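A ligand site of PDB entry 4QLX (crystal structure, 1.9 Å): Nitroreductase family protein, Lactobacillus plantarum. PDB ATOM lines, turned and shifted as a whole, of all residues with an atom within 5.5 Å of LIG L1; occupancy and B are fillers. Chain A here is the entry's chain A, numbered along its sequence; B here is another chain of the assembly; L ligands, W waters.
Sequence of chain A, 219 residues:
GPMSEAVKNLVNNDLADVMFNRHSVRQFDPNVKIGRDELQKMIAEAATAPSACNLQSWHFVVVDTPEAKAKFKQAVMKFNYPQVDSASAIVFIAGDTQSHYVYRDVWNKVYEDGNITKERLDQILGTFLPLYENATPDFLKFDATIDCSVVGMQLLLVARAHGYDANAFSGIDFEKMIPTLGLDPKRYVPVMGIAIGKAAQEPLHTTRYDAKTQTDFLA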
ATOM      1  N   SER A  51      26.594 -11.200 -15.369  1.00  0.00           N
ATOM      2  CA  SER A  51      25.160 -11.199 -15.589  1.00  0.00           C
ATOM      3  C   SER A  51      24.640  -9.934 -14.939  1.00  0.00           C
ATOM      4  O   SER A  51      25.239  -9.445 -13.965  1.00  0.00           O
ATOM      5  CB  SER A  51      24.487 -12.460 -15.003  1.00  0.00           C
ATOM      6  OG  SER A  51      24.623 -12.480 -13.587  1.00  0.00           O
ATOM      7  N   ALA A  52      23.563  -9.370 -15.475  1.00  0.00           N
ATOM      8  CA  ALA A  52      23.031  -8.133 -14.901  1.00  0.00           C
ATOM      9  C   ALA A  52      22.632  -8.362 -13.450  1.00  0.00           C
ATOM     10  O   ALA A  52      21.917  -9.310 -13.126  1.00  0.00           O
ATOM     11  CB  ALA A  52      21.828  -7.616 -15.710  1.00  0.00           C
ATOM     12  N   CYS A  53      23.138  -7.499 -12.572  1.00  0.00           N
ATOM     13  CA  CYS A  53      22.922  -7.588 -11.115  1.00  0.00           C
ATOM     14  C   CYS A  53      23.241  -8.960 -10.524  1.00  0.00           C
ATOM     15  O   CYS A  53      22.669  -9.346  -9.498  1.00  0.00           O
ATOM     16  CB  CYS A  53      21.479  -7.209 -10.779  1.00  0.00           C
ATOM     17  SG  CYS A  53      21.146  -5.436 -11.010  1.00  0.00           S
ATOM     18  N   ASN A  54      24.168  -9.669 -11.165  1.00  0.00           N
ATOM     19  CA  ASN A  54      24.564 -11.028 -10.777  1.00  0.00           C
ATOM     20  C   ASN A  54      23.377 -11.966 -10.577  1.00  0.00           C
ATOM     21  O   ASN A  54      23.447 -12.909  -9.797  1.00  0.00           O
ATOM     22  CB  ASN A  54      25.442 -11.018  -9.505  1.00  0.00           C
ATOM     23  CG  ASN A  54      26.271 -12.304  -9.358  1.00  0.00           C
ATOM     24  OD1 ASN A  54      26.605 -12.945 -10.357  1.00  0.00           O
ATOM     25  ND2 ASN A  54      26.572 -12.680  -8.125  1.00  0.00           N
ATOM     26  N   TYR A 103      16.342 -11.004  -5.839  1.00  0.00           N
ATOM     27  CA  TYR A 103      17.262  -9.859  -5.873  1.00  0.00           C
ATOM     28  C   TYR A 103      17.621  -9.377  -4.462  1.00  0.00           C
ATOM     29  O   TYR A 103      18.793  -9.340  -4.097  1.00  0.00           O
ATOM     30  CB  TYR A 103      16.647  -8.710  -6.684  1.00  0.00           C
ATOM     31  CG  TYR A 103      17.612  -7.570  -7.004  1.00  0.00           C
ATOM     32  CD1 TYR A 103      18.119  -6.743  -5.994  1.00  0.00           C
ATOM     33  CD2 TYR A 103      17.991  -7.307  -8.297  1.00  0.00           C
ATOM     34  CE1 TYR A 103      18.999  -5.701  -6.282  1.00  0.00           C
ATOM     35  CE2 TYR A 103      18.862  -6.273  -8.590  1.00  0.00           C
ATOM     36  CZ  TYR A 103      19.368  -5.477  -7.584  1.00  0.00           C
ATOM     37  OH  TYR A 103      20.234  -4.465  -7.887  1.00  0.00           O
ATOM     38  N   TRP A 107      21.485  -9.763  -2.668  1.00  0.00           N
ATOM     39  CA  TRP A 107      22.401  -8.668  -2.394  1.00  0.00           C
ATOM     40  C   TRP A 107      22.493  -8.410  -0.870  1.00  0.00           C
ATOM     41  O   TRP A 107      23.486  -7.884  -0.372  1.00  0.00           O
ATOM     42  CB  TRP A 107      22.007  -7.420  -3.198  1.00  0.00           C
ATOM     43  CG  TRP A 107      22.481  -7.624  -4.610  1.00  0.00           C
ATOM     44  CD1 TRP A 107      21.735  -7.963  -5.710  1.00  0.00           C
ATOM     45  CD2 TRP A 107      23.845  -7.584  -5.047  1.00  0.00           C
ATOM     46  NE1 TRP A 107      22.547  -8.116  -6.815  1.00  0.00           N
ATOM     47  CE2 TRP A 107      23.852  -7.896  -6.434  1.00  0.00           C
ATOM     48  CE3 TRP A 107      25.060  -7.303  -4.414  1.00  0.00           C
ATOM     49  CZ2 TRP A 107      25.018  -7.917  -7.179  1.00  0.00           C
ATOM     50  CZ3 TRP A 107      26.225  -7.353  -5.163  1.00  0.00           C
ATOM     51  CH2 TRP A 107      26.198  -7.644  -6.526  1.00  0.00           C
ATOM     52  N   ILE A 116      30.125  -5.804   1.259  1.00  0.00           N
ATOM     53  CA  ILE A 116      29.758  -4.430   0.909  1.00  0.00           C
ATOM     54  C   ILE A 116      29.216  -3.729   2.143  1.00  0.00           C
ATOM     55  O   ILE A 116      28.744  -4.369   3.089  1.00  0.00           O
ATOM     56  CB  ILE A 116      28.686  -4.355  -0.228  1.00  0.00           C
ATOM     57  CG1 ILE A 116      27.405  -5.060   0.184  1.00  0.00           C
ATOM     58  CG2 ILE A 116      29.231  -4.927  -1.535  1.00  0.00           C
ATOM     59  CD1 ILE A 116      26.279  -4.899  -0.803  1.00  0.00           C
ATOM     60  N   ARG A 120      26.309   0.991   0.539  1.00  0.00           N
ATOM     61  CA  ARG A 120      26.454   0.433  -0.803  1.00  0.00           C
ATOM     62  C   ARG A 120      25.242  -0.441  -1.157  1.00  0.00           C
ATOM     63  O   ARG A 120      24.640  -0.275  -2.224  1.00  0.00           O
ATOM     64  CB  ARG A 120      27.762  -0.370  -0.901  1.00  0.00           C
ATOM     65  CG  ARG A 120      28.152  -0.760  -2.319  1.00  0.00           C
ATOM     66  CD  ARG A 120      28.061   0.443  -3.255  1.00  0.00           C
ATOM     67  NE  ARG A 120      28.705   0.191  -4.549  1.00  0.00           N
ATOM     68  CZ  ARG A 120      28.423   0.874  -5.648  1.00  0.00           C
ATOM     69  NH1 ARG A 120      27.512   1.832  -5.625  1.00  0.00           N
ATOM     70  NH2 ARG A 120      29.056   0.581  -6.784  1.00  0.00           N
ATOM     71  N   ILE A 124      22.471  -0.158  -4.272  1.00  0.00           N
ATOM     72  CA  ILE A 124      22.187  -1.256  -5.213  1.00  0.00           C
ATOM     73  C   ILE A 124      20.694  -1.615  -5.230  1.00  0.00           C
ATOM     74  O   ILE A 124      20.098  -1.734  -6.291  1.00  0.00           O
ATOM     75  CB  ILE A 124      23.016  -2.503  -4.875  1.00  0.00           C
ATOM     76  CG1 ILE A 124      24.512  -2.174  -4.887  1.00  0.00           C
ATOM     77  CG2 ILE A 124      22.725  -3.651  -5.867  1.00  0.00           C
ATOM     78  CD1 ILE A 124      25.383  -3.291  -4.361  1.00  0.00           C
ATOM     79  N   PHE A 128      18.333  -0.485  -8.765  1.00  0.00           N
ATOM     80  CA  PHE A 128      18.015  -1.429  -9.829  1.00  0.00           C
ATOM     81  C   PHE A 128      16.823  -2.340  -9.538  1.00  0.00           C
ATOM     82  O   PHE A 128      16.142  -2.766 -10.478  1.00  0.00           O
ATOM     83  CB  PHE A 128      19.250  -2.278 -10.144  1.00  0.00           C
ATOM     84  CG  PHE A 128      20.388  -1.465 -10.691  1.00  0.00           C
ATOM     85  CD1 PHE A 128      20.344  -1.008 -12.003  1.00  0.00           C
ATOM     86  CD2 PHE A 128      21.464  -1.128  -9.895  1.00  0.00           C
ATOM     87  CE1 PHE A 128      21.380  -0.245 -12.511  1.00  0.00           C
ATOM     88  CE2 PHE A 128      22.513  -0.369 -10.401  1.00  0.00           C
ATOM     89  CZ  PHE A 128      22.465   0.077 -11.706  1.00  0.00           C
ATOM     90  N   LEU A 131      13.506  -1.167 -10.980  1.00  0.00           N
ATOM     91  CA  LEU A 131      13.446  -1.336 -12.433  1.00  0.00           C
ATOM     92  C   LEU A 131      13.053  -2.760 -12.831  1.00  0.00           C
ATOM     93  O   LEU A 131      12.376  -2.973 -13.838  1.00  0.00           O
ATOM     94  CB  LEU A 131      14.792  -0.974 -13.079  1.00  0.00           C
ATOM     95  CG  LEU A 131      15.013   0.502 -13.433  1.00  0.00           C
ATOM     96  CD1 LEU A 131      14.853   1.396 -12.238  1.00  0.00           C
ATOM     97  CD2 LEU A 131      16.384   0.681 -14.057  1.00  0.00           C
ATOM     98  N   TYR A 132      13.517  -3.732 -12.056  1.00  0.00           N
ATOM     99  CA  TYR A 132      13.135  -5.120 -12.300  1.00  0.00           C
ATOM    100  C   TYR A 132      11.682  -5.319 -11.885  1.00  0.00           C
ATOM    101  O   TYR A 132      10.920  -6.023 -12.555  1.00  0.00           O
ATOM    102  CB  TYR A 132      14.055  -6.089 -11.539  1.00  0.00           C
ATOM    103  CG  TYR A 132      15.338  -6.408 -12.263  1.00  0.00           C
ATOM    104  CD1 TYR A 132      15.340  -7.187 -13.416  1.00  0.00           C
ATOM    105  CD2 TYR A 132      16.567  -5.949 -11.782  1.00  0.00           C
ATOM    106  CE1 TYR A 132      16.519  -7.480 -14.080  1.00  0.00           C
ATOM    107  CE2 TYR A 132      17.733  -6.227 -12.431  1.00  0.00           C
ATOM    108  CZ  TYR A 132      17.709  -6.992 -13.580  1.00  0.00           C
ATOM    109  OH  TYR A 132      18.892  -7.287 -14.231  1.00  0.00           O
ATOM    110  N   ALA A 135       9.251  -3.773 -14.445  1.00  0.00           N
ATOM    111  CA  ALA A 135       9.663  -4.020 -15.825  1.00  0.00           C
ATOM    112  C   ALA A 135       8.586  -4.723 -16.633  1.00  0.00           C
ATOM    113  O   ALA A 135       7.884  -5.588 -16.125  1.00  0.00           O
ATOM    114  CB  ALA A 135      10.966  -4.837 -15.854  1.00  0.00           C
ATOM    115  N   PHE A 139      11.137  -6.350 -21.584  1.00  0.00           N
ATOM    116  CA  PHE A 139      12.410  -5.950 -21.007  1.00  0.00           C
ATOM    117  C   PHE A 139      13.060  -7.028 -20.136  1.00  0.00           C
ATOM    118  O   PHE A 139      14.280  -7.116 -20.063  1.00  0.00           O
ATOM    119  CB  PHE A 139      12.279  -4.673 -20.184  1.00  0.00           C
ATOM    120  CG  PHE A 139      13.599  -4.078 -19.809  1.00  0.00           C
ATOM    121  CD1 PHE A 139      14.325  -3.320 -20.727  1.00  0.00           C
ATOM    122  CD2 PHE A 139      14.142  -4.302 -18.545  1.00  0.00           C
ATOM    123  CE1 PHE A 139      15.557  -2.788 -20.390  1.00  0.00           C
ATOM    124  CE2 PHE A 139      15.374  -3.771 -18.208  1.00  0.00           C
ATOM    125  CZ  PHE A 139      16.087  -3.009 -19.127  1.00  0.00           C
ATOM    126  N   ASP A 143      16.662  -8.568 -20.934  1.00  0.00           N
ATOM    127  CA  ASP A 143      17.644  -8.734 -19.876  1.00  0.00           C
ATOM    128  C   ASP A 143      18.128 -10.187 -19.791  1.00  0.00           C
ATOM    129  O   ASP A 143      19.325 -10.467 -19.747  1.00  0.00           O
ATOM    130  CB  ASP A 143      17.027  -8.293 -18.539  1.00  0.00           C
ATOM    131  CG  ASP A 143      17.956  -8.523 -17.341  1.00  0.00           C
ATOM    132  OD1 ASP A 143      17.961  -9.635 -16.770  1.00  0.00           O
ATOM    133  OD2 ASP A 143      18.656  -7.553 -16.949  1.00  0.00           O
ATOM    134  N   ARG B  26      35.192  -1.356 -11.660  1.00  0.00           N
ATOM    135  CA  ARG B  26      34.383  -0.146 -11.843  1.00  0.00           C
ATOM    136  C   ARG B  26      35.180   1.127 -11.571  1.00  0.00           C
ATOM    137  O   ARG B  26      34.844   2.196 -12.035  1.00  0.00           O
ATOM    138  CB  ARG B  26      33.143  -0.198 -10.927  1.00  0.00           C
ATOM    139  CG  ARG B  26      32.165  -1.324 -11.297  1.00  0.00           C
ATOM    140  CD  ARG B  26      30.995  -1.477 -10.294  1.00  0.00           C
ATOM    141  NE  ARG B  26      30.085  -2.529 -10.741  1.00  0.00           N
ATOM    142  CZ  ARG B  26      30.239  -3.826 -10.464  1.00  0.00           C
ATOM    143  NH1 ARG B  26      31.257  -4.245  -9.722  1.00  0.00           N
ATOM    144  NH2 ARG B  26      29.367  -4.718 -10.945  1.00  0.00           N
ATOM    145  N   PHE B  79      24.464   5.780 -11.202  1.00  0.00           N
ATOM    146  CA  PHE B  79      25.131   4.660 -10.543  1.00  0.00           C
ATOM    147  C   PHE B  79      26.412   4.281 -11.276  1.00  0.00           C
ATOM    148  O   PHE B  79      27.392   3.879 -10.662  1.00  0.00           O
ATOM    149  CB  PHE B  79      24.189   3.441 -10.460  1.00  0.00           C
ATOM    150  CG  PHE B  79      24.753   2.278  -9.684  1.00  0.00           C
ATOM    151  CD1 PHE B  79      25.611   1.371 -10.300  1.00  0.00           C
ATOM    152  CD2 PHE B  79      24.413   2.087  -8.357  1.00  0.00           C
ATOM    153  CE1 PHE B  79      26.125   0.292  -9.576  1.00  0.00           C
ATOM    154  CE2 PHE B  79      24.936   1.011  -7.636  1.00  0.00           C
ATOM    155  CZ  PHE B  79      25.781   0.114  -8.245  1.00  0.00           C
ATOM    156  N   PHE B 169      28.023  -2.881 -18.693  1.00  0.00           N
ATOM    157  CA  PHE B 169      26.900  -2.282 -17.994  1.00  0.00           C
ATOM    158  C   PHE B 169      25.736  -1.927 -18.890  1.00  0.00           C
ATOM    159  O   PHE B 169      25.918  -1.507 -20.035  1.00  0.00           O
ATOM    160  CB  PHE B 169      27.358  -1.034 -17.196  1.00  0.00           C
ATOM    161  CG  PHE B 169      27.856   0.093 -18.043  1.00  0.00           C
ATOM    162  CD1 PHE B 169      29.193   0.183 -18.392  1.00  0.00           C
ATOM    163  CD2 PHE B 169      26.987   1.085 -18.475  1.00  0.00           C
ATOM    164  CE1 PHE B 169      29.648   1.217 -19.176  1.00  0.00           C
ATOM    165  CE2 PHE B 169      27.442   2.129 -19.242  1.00  0.00           C
ATOM    166  CZ  PHE B 169      28.774   2.192 -19.609  1.00  0.00           C
ATOM    167  N   SER B 170      24.526  -2.111 -18.367  1.00  0.00           N
ATOM    168  CA  SER B 170      23.336  -1.786 -19.135  1.00  0.00           C
ATOM    169  C   SER B 170      22.419  -0.852 -18.354  1.00  0.00           C
ATOM    170  O   SER B 170      21.284  -0.603 -18.764  1.00  0.00           O
ATOM    171  CB  SER B 170      22.586  -3.060 -19.540  1.00  0.00           C
ATOM    172  OG  SER B 170      22.067  -3.749 -18.416  1.00  0.00           O
ATOM    173  N   GLY B 171      22.921  -0.343 -17.232  1.00  0.00           N
ATOM    174  CA  GLY B 171      22.210   0.671 -16.480  1.00  0.00           C
ATOM    175  C   GLY B 171      22.267   1.991 -17.225  1.00  0.00           C
ATOM    176  O   GLY B 171      23.097   2.867 -16.899  1.00  0.00           O
ATOM    177  N   PHE B 174      17.322   3.760 -21.966  1.00  0.00           N
ATOM    178  CA  PHE B 174      17.190   3.031 -23.228  1.00  0.00           C
ATOM    179  C   PHE B 174      16.487   3.868 -24.286  1.00  0.00           C
ATOM    180  O   PHE B 174      16.667   3.629 -25.467  1.00  0.00           O
ATOM    181  CB  PHE B 174      16.464   1.700 -23.000  1.00  0.00           C
ATOM    182  CG  PHE B 174      17.253   0.728 -22.159  1.00  0.00           C
ATOM    183  CD1 PHE B 174      17.166   0.768 -20.769  1.00  0.00           C
ATOM    184  CD2 PHE B 174      18.117  -0.175 -22.753  1.00  0.00           C
ATOM    185  CE1 PHE B 174      17.904  -0.102 -19.991  1.00  0.00           C
ATOM    186  CE2 PHE B 174      18.860  -1.058 -21.979  1.00  0.00           C
ATOM    187  CZ  PHE B 174      18.750  -1.018 -20.588  1.00  0.00           C
HETATM  188  O1  LIG L   1      31.963  -2.614  -5.984  1.00  0.00           O
HETATM  189  C1  LIG L   1      31.155  -2.633  -5.053  1.00  0.00           C
HETATM  190  O2  LIG L   1      31.377  -1.879  -3.968  1.00  0.00           O
HETATM  191  C2  LIG L   1      29.920  -3.494  -5.151  1.00  0.00           C
HETATM  192  C3  LIG L   1      29.551  -3.604  -6.613  1.00  0.00           C
HETATM  193  C4  LIG L   1      28.093  -3.243  -6.804  1.00  0.00           C
HETATM  194  C5  LIG L   1      27.342  -4.485  -7.242  1.00  0.00           C
HETATM  195  C6  LIG L   1      26.862  -4.324  -8.671  1.00  0.00           C
HETATM  196  C7  LIG L   1      25.519  -3.649  -8.703  1.00  0.00           C
HETATM  197  C8  LIG L   1      24.718  -4.227  -9.858  1.00  0.00           C
HETATM  198  C9  LIG L   1      24.771  -3.311 -11.058  1.00  0.00           C
HETATM  199  C10 LIG L   1      24.165  -4.041 -12.221  1.00  0.00           C
HETATM  200  O3  LIG L   1      24.583  -5.156 -12.508  1.00  0.00           O
HETATM  201  C11 LIG L   1      23.052  -3.377 -12.987  1.00  0.00           C
HETATM  202  C12 LIG L   1      22.693  -4.223 -14.195  1.00  0.00           C
HETATM  203  C13 LIG L   1      21.954  -3.400 -15.242  1.00  0.00           C
HETATM  204  C14 LIG L   1      20.454  -3.574 -15.081  1.00  0.00           C
HETATM  205  C15 LIG L   1      19.694  -2.745 -16.118  1.00  0.00           C
HETATM  206  C16 LIG L   1      18.230  -2.569 -15.684  1.00  0.00           C
HETATM  207  C17 LIG L   1      17.674  -3.891 -15.161  1.00  0.00           C
HETATM  208  C18 LIG L   1      16.205  -3.805 -14.824  1.00  0.00           C
HETATM  209  N1  LG2 L   2      27.557  -3.417 -13.248  1.00  0.00           N
HETATM  210  C1  LG2 L   2      27.327  -2.114 -12.842  1.00  0.00           C
HETATM  211  O1  LG2 L   2      27.986  -1.640 -11.909  1.00  0.00           O
HETATM  212  N2  LG2 L   2      26.357  -1.348 -13.456  1.00  0.00           N
HETATM  213  C2  LG2 L   2      25.607  -1.875 -14.492  1.00  0.00           C
HETATM  214  O2  LG2 L   2      24.750  -1.205 -15.050  1.00  0.00           O
HETATM  215  C3  LG2 L   2      25.841  -3.167 -14.906  1.00  0.00           C
HETATM  216  N3  LG2 L   2      25.092  -3.669 -15.946  1.00  0.00           N
HETATM  217  C4  LG2 L   2      25.312  -4.954 -16.399  1.00  0.00           C
HETATM  218  C5  LG2 L   2      24.553  -5.423 -17.461  1.00  0.00           C
HETATM  219  C6  LG2 L   2      24.767  -6.706 -17.927  1.00  0.00           C
HETATM  220  C7  LG2 L   2      23.963  -7.242 -19.074  1.00  0.00           C
HETATM  221  C8  LG2 L   2      25.748  -7.503 -17.353  1.00  0.00           C
HETATM  222  C9  LG2 L   2      25.950  -8.882 -17.875  1.00  0.00           C
HETATM  223  C10 LG2 L   2      26.508  -7.023 -16.274  1.00  0.00           C
HETATM  224  C11 LG2 L   2      26.299  -5.743 -15.796  1.00  0.00           C
HETATM  225  N4  LG2 L   2      27.028  -5.236 -14.708  1.00  0.00           N
HETATM  226  C12 LG2 L   2      26.816  -3.945 -14.296  1.00  0.00           C
HETATM  227  C13 LG2 L   2      28.094  -6.051 -14.033  1.00  0.00           C
HETATM  228  C14 LG2 L   2      27.447  -7.074 -13.066  1.00  0.00           C
HETATM  229  O3  LG2 L   2      26.901  -6.428 -11.915  1.00  0.00           O
HETATM  230  C15 LG2 L   2      28.431  -8.192 -12.714  1.00  0.00           C
HETATM  231  O4  LG2 L   2      28.746  -8.932 -13.897  1.00  0.00           O
HETATM  232  C16 LG2 L   2      27.903  -9.210 -11.684  1.00  0.00           C
HETATM  233  O5  LG2 L   2      27.732  -8.629 -10.428  1.00  0.00           O
HETATM  234  C17 LG2 L   2      28.859 -10.393 -11.539  1.00  0.00           C
HETATM  235  O6  LG2 L   2      30.109  -9.902 -11.092  1.00  0.00           O
HETATM  236  P1  LG2 L   2      31.473 -10.106 -11.944  1.00  0.00           P
HETATM  237  O7  LG2 L   2      31.754 -11.577 -12.159  1.00  0.00           O
HETATM  238  O8  LG2 L   2      31.328  -9.451 -13.285  1.00  0.00           O
HETATM  239  O9  LG2 L   2      32.590  -9.445 -11.135  1.00  0.00           O
HETATM  240  O   HOH W   1      33.549  -2.698  -8.098  1.00  0.00           O
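The guanidinium group (NE) of Arg 26 of chain B sits at hydrogen-bond distance from an oxygen (O1) of LG2 L2.
The backbone NH (N) of Gly 171 of chain B lies within hydrogen-bond range of an oxygen (O2) of LG2 L2, 3.0 Å away.
The backbone NH (N) of Ser 51 sits at hydrogen-bond distance from an oxygen (O4) of LG2 L2, 3.5 Å away.
N of Cys 53 lies within hydrogen-bond range of O3 of LIG L1, 2.8 Å away.
A nitrogen (N3) of LG2 L2 lies within hydrogen-bond range of the backbone NH of Ser 170 of chain B, at 2.9 Å.
The side-chain sulfur of Cys 53 lies close to an oxygen (O3) of LIG L1, at 3.8 Å.
An oxygen (O2) of LIG L1 lies within salt-bridge range of the guanidinium group of Arg 120 (3.4 Å).
Ala 52 touches LIG L1.
Trp 107 touches LIG L1.
CG2 of Ile 116 touches C2 of LIG L1, at 3.95 Å.
CD1 of Ile 124 touches C4 of LIG L1 (3.6 Å).
CE1 of Phe 128 touches C11 of LIG L1, at 3.6 Å.
CB of Leu 131 touches C18 of LIG L1, 3.6 Å away.
Tyr 132 touches LIG L1.
CE2 of Phe 139 touches C18 of LIG L1 (3.5 Å).
Arg 26 of chain B touches LIG L1 (NH2 to C6, 3.4 Å).
CZ of Phe 79 of chain B touches C7 of LIG L1, at 3.8 Å.
Ser 170 of chain B touches LIG L1.
Gly 171 of chain B touches LIG L1.
Hydrophobic or aromatic side chains that line LIG L1: Ala 52, Trp 107, Ile 116, Ile 124, Phe 128, Leu 131, Tyr 132, Phe 139 and Phe 79 of chain B.
Water W1 lies within hydrogen-bond range of an oxygen (O1) of LIG L1 (2.6 Å) and the guanidinium group of Arg 26 of chain B (3.2 Å).
OH of Tyr 103 lies within hydrogen-bond range of SG of Cys 53 (3.4 Å).
The backbone carbonyl oxygen (O) of Cys 53 lies within hydrogen-bond range of the indole nitrogen (NE1) of Trp 107.
The backbone carbonyl oxygen (O) of Ile 124 is in hydrogen-bond range of the side-chain hydroxyl (OH) of Tyr 103 (3.2 Å).
OD2 of Asp 143 lies within hydrogen-bond range of OH of Tyr 132.
An oxygen (O3) of LIG L1 is in hydrogen-bond range of an oxygen (O3) of LG2 L2 (2.7 Å).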
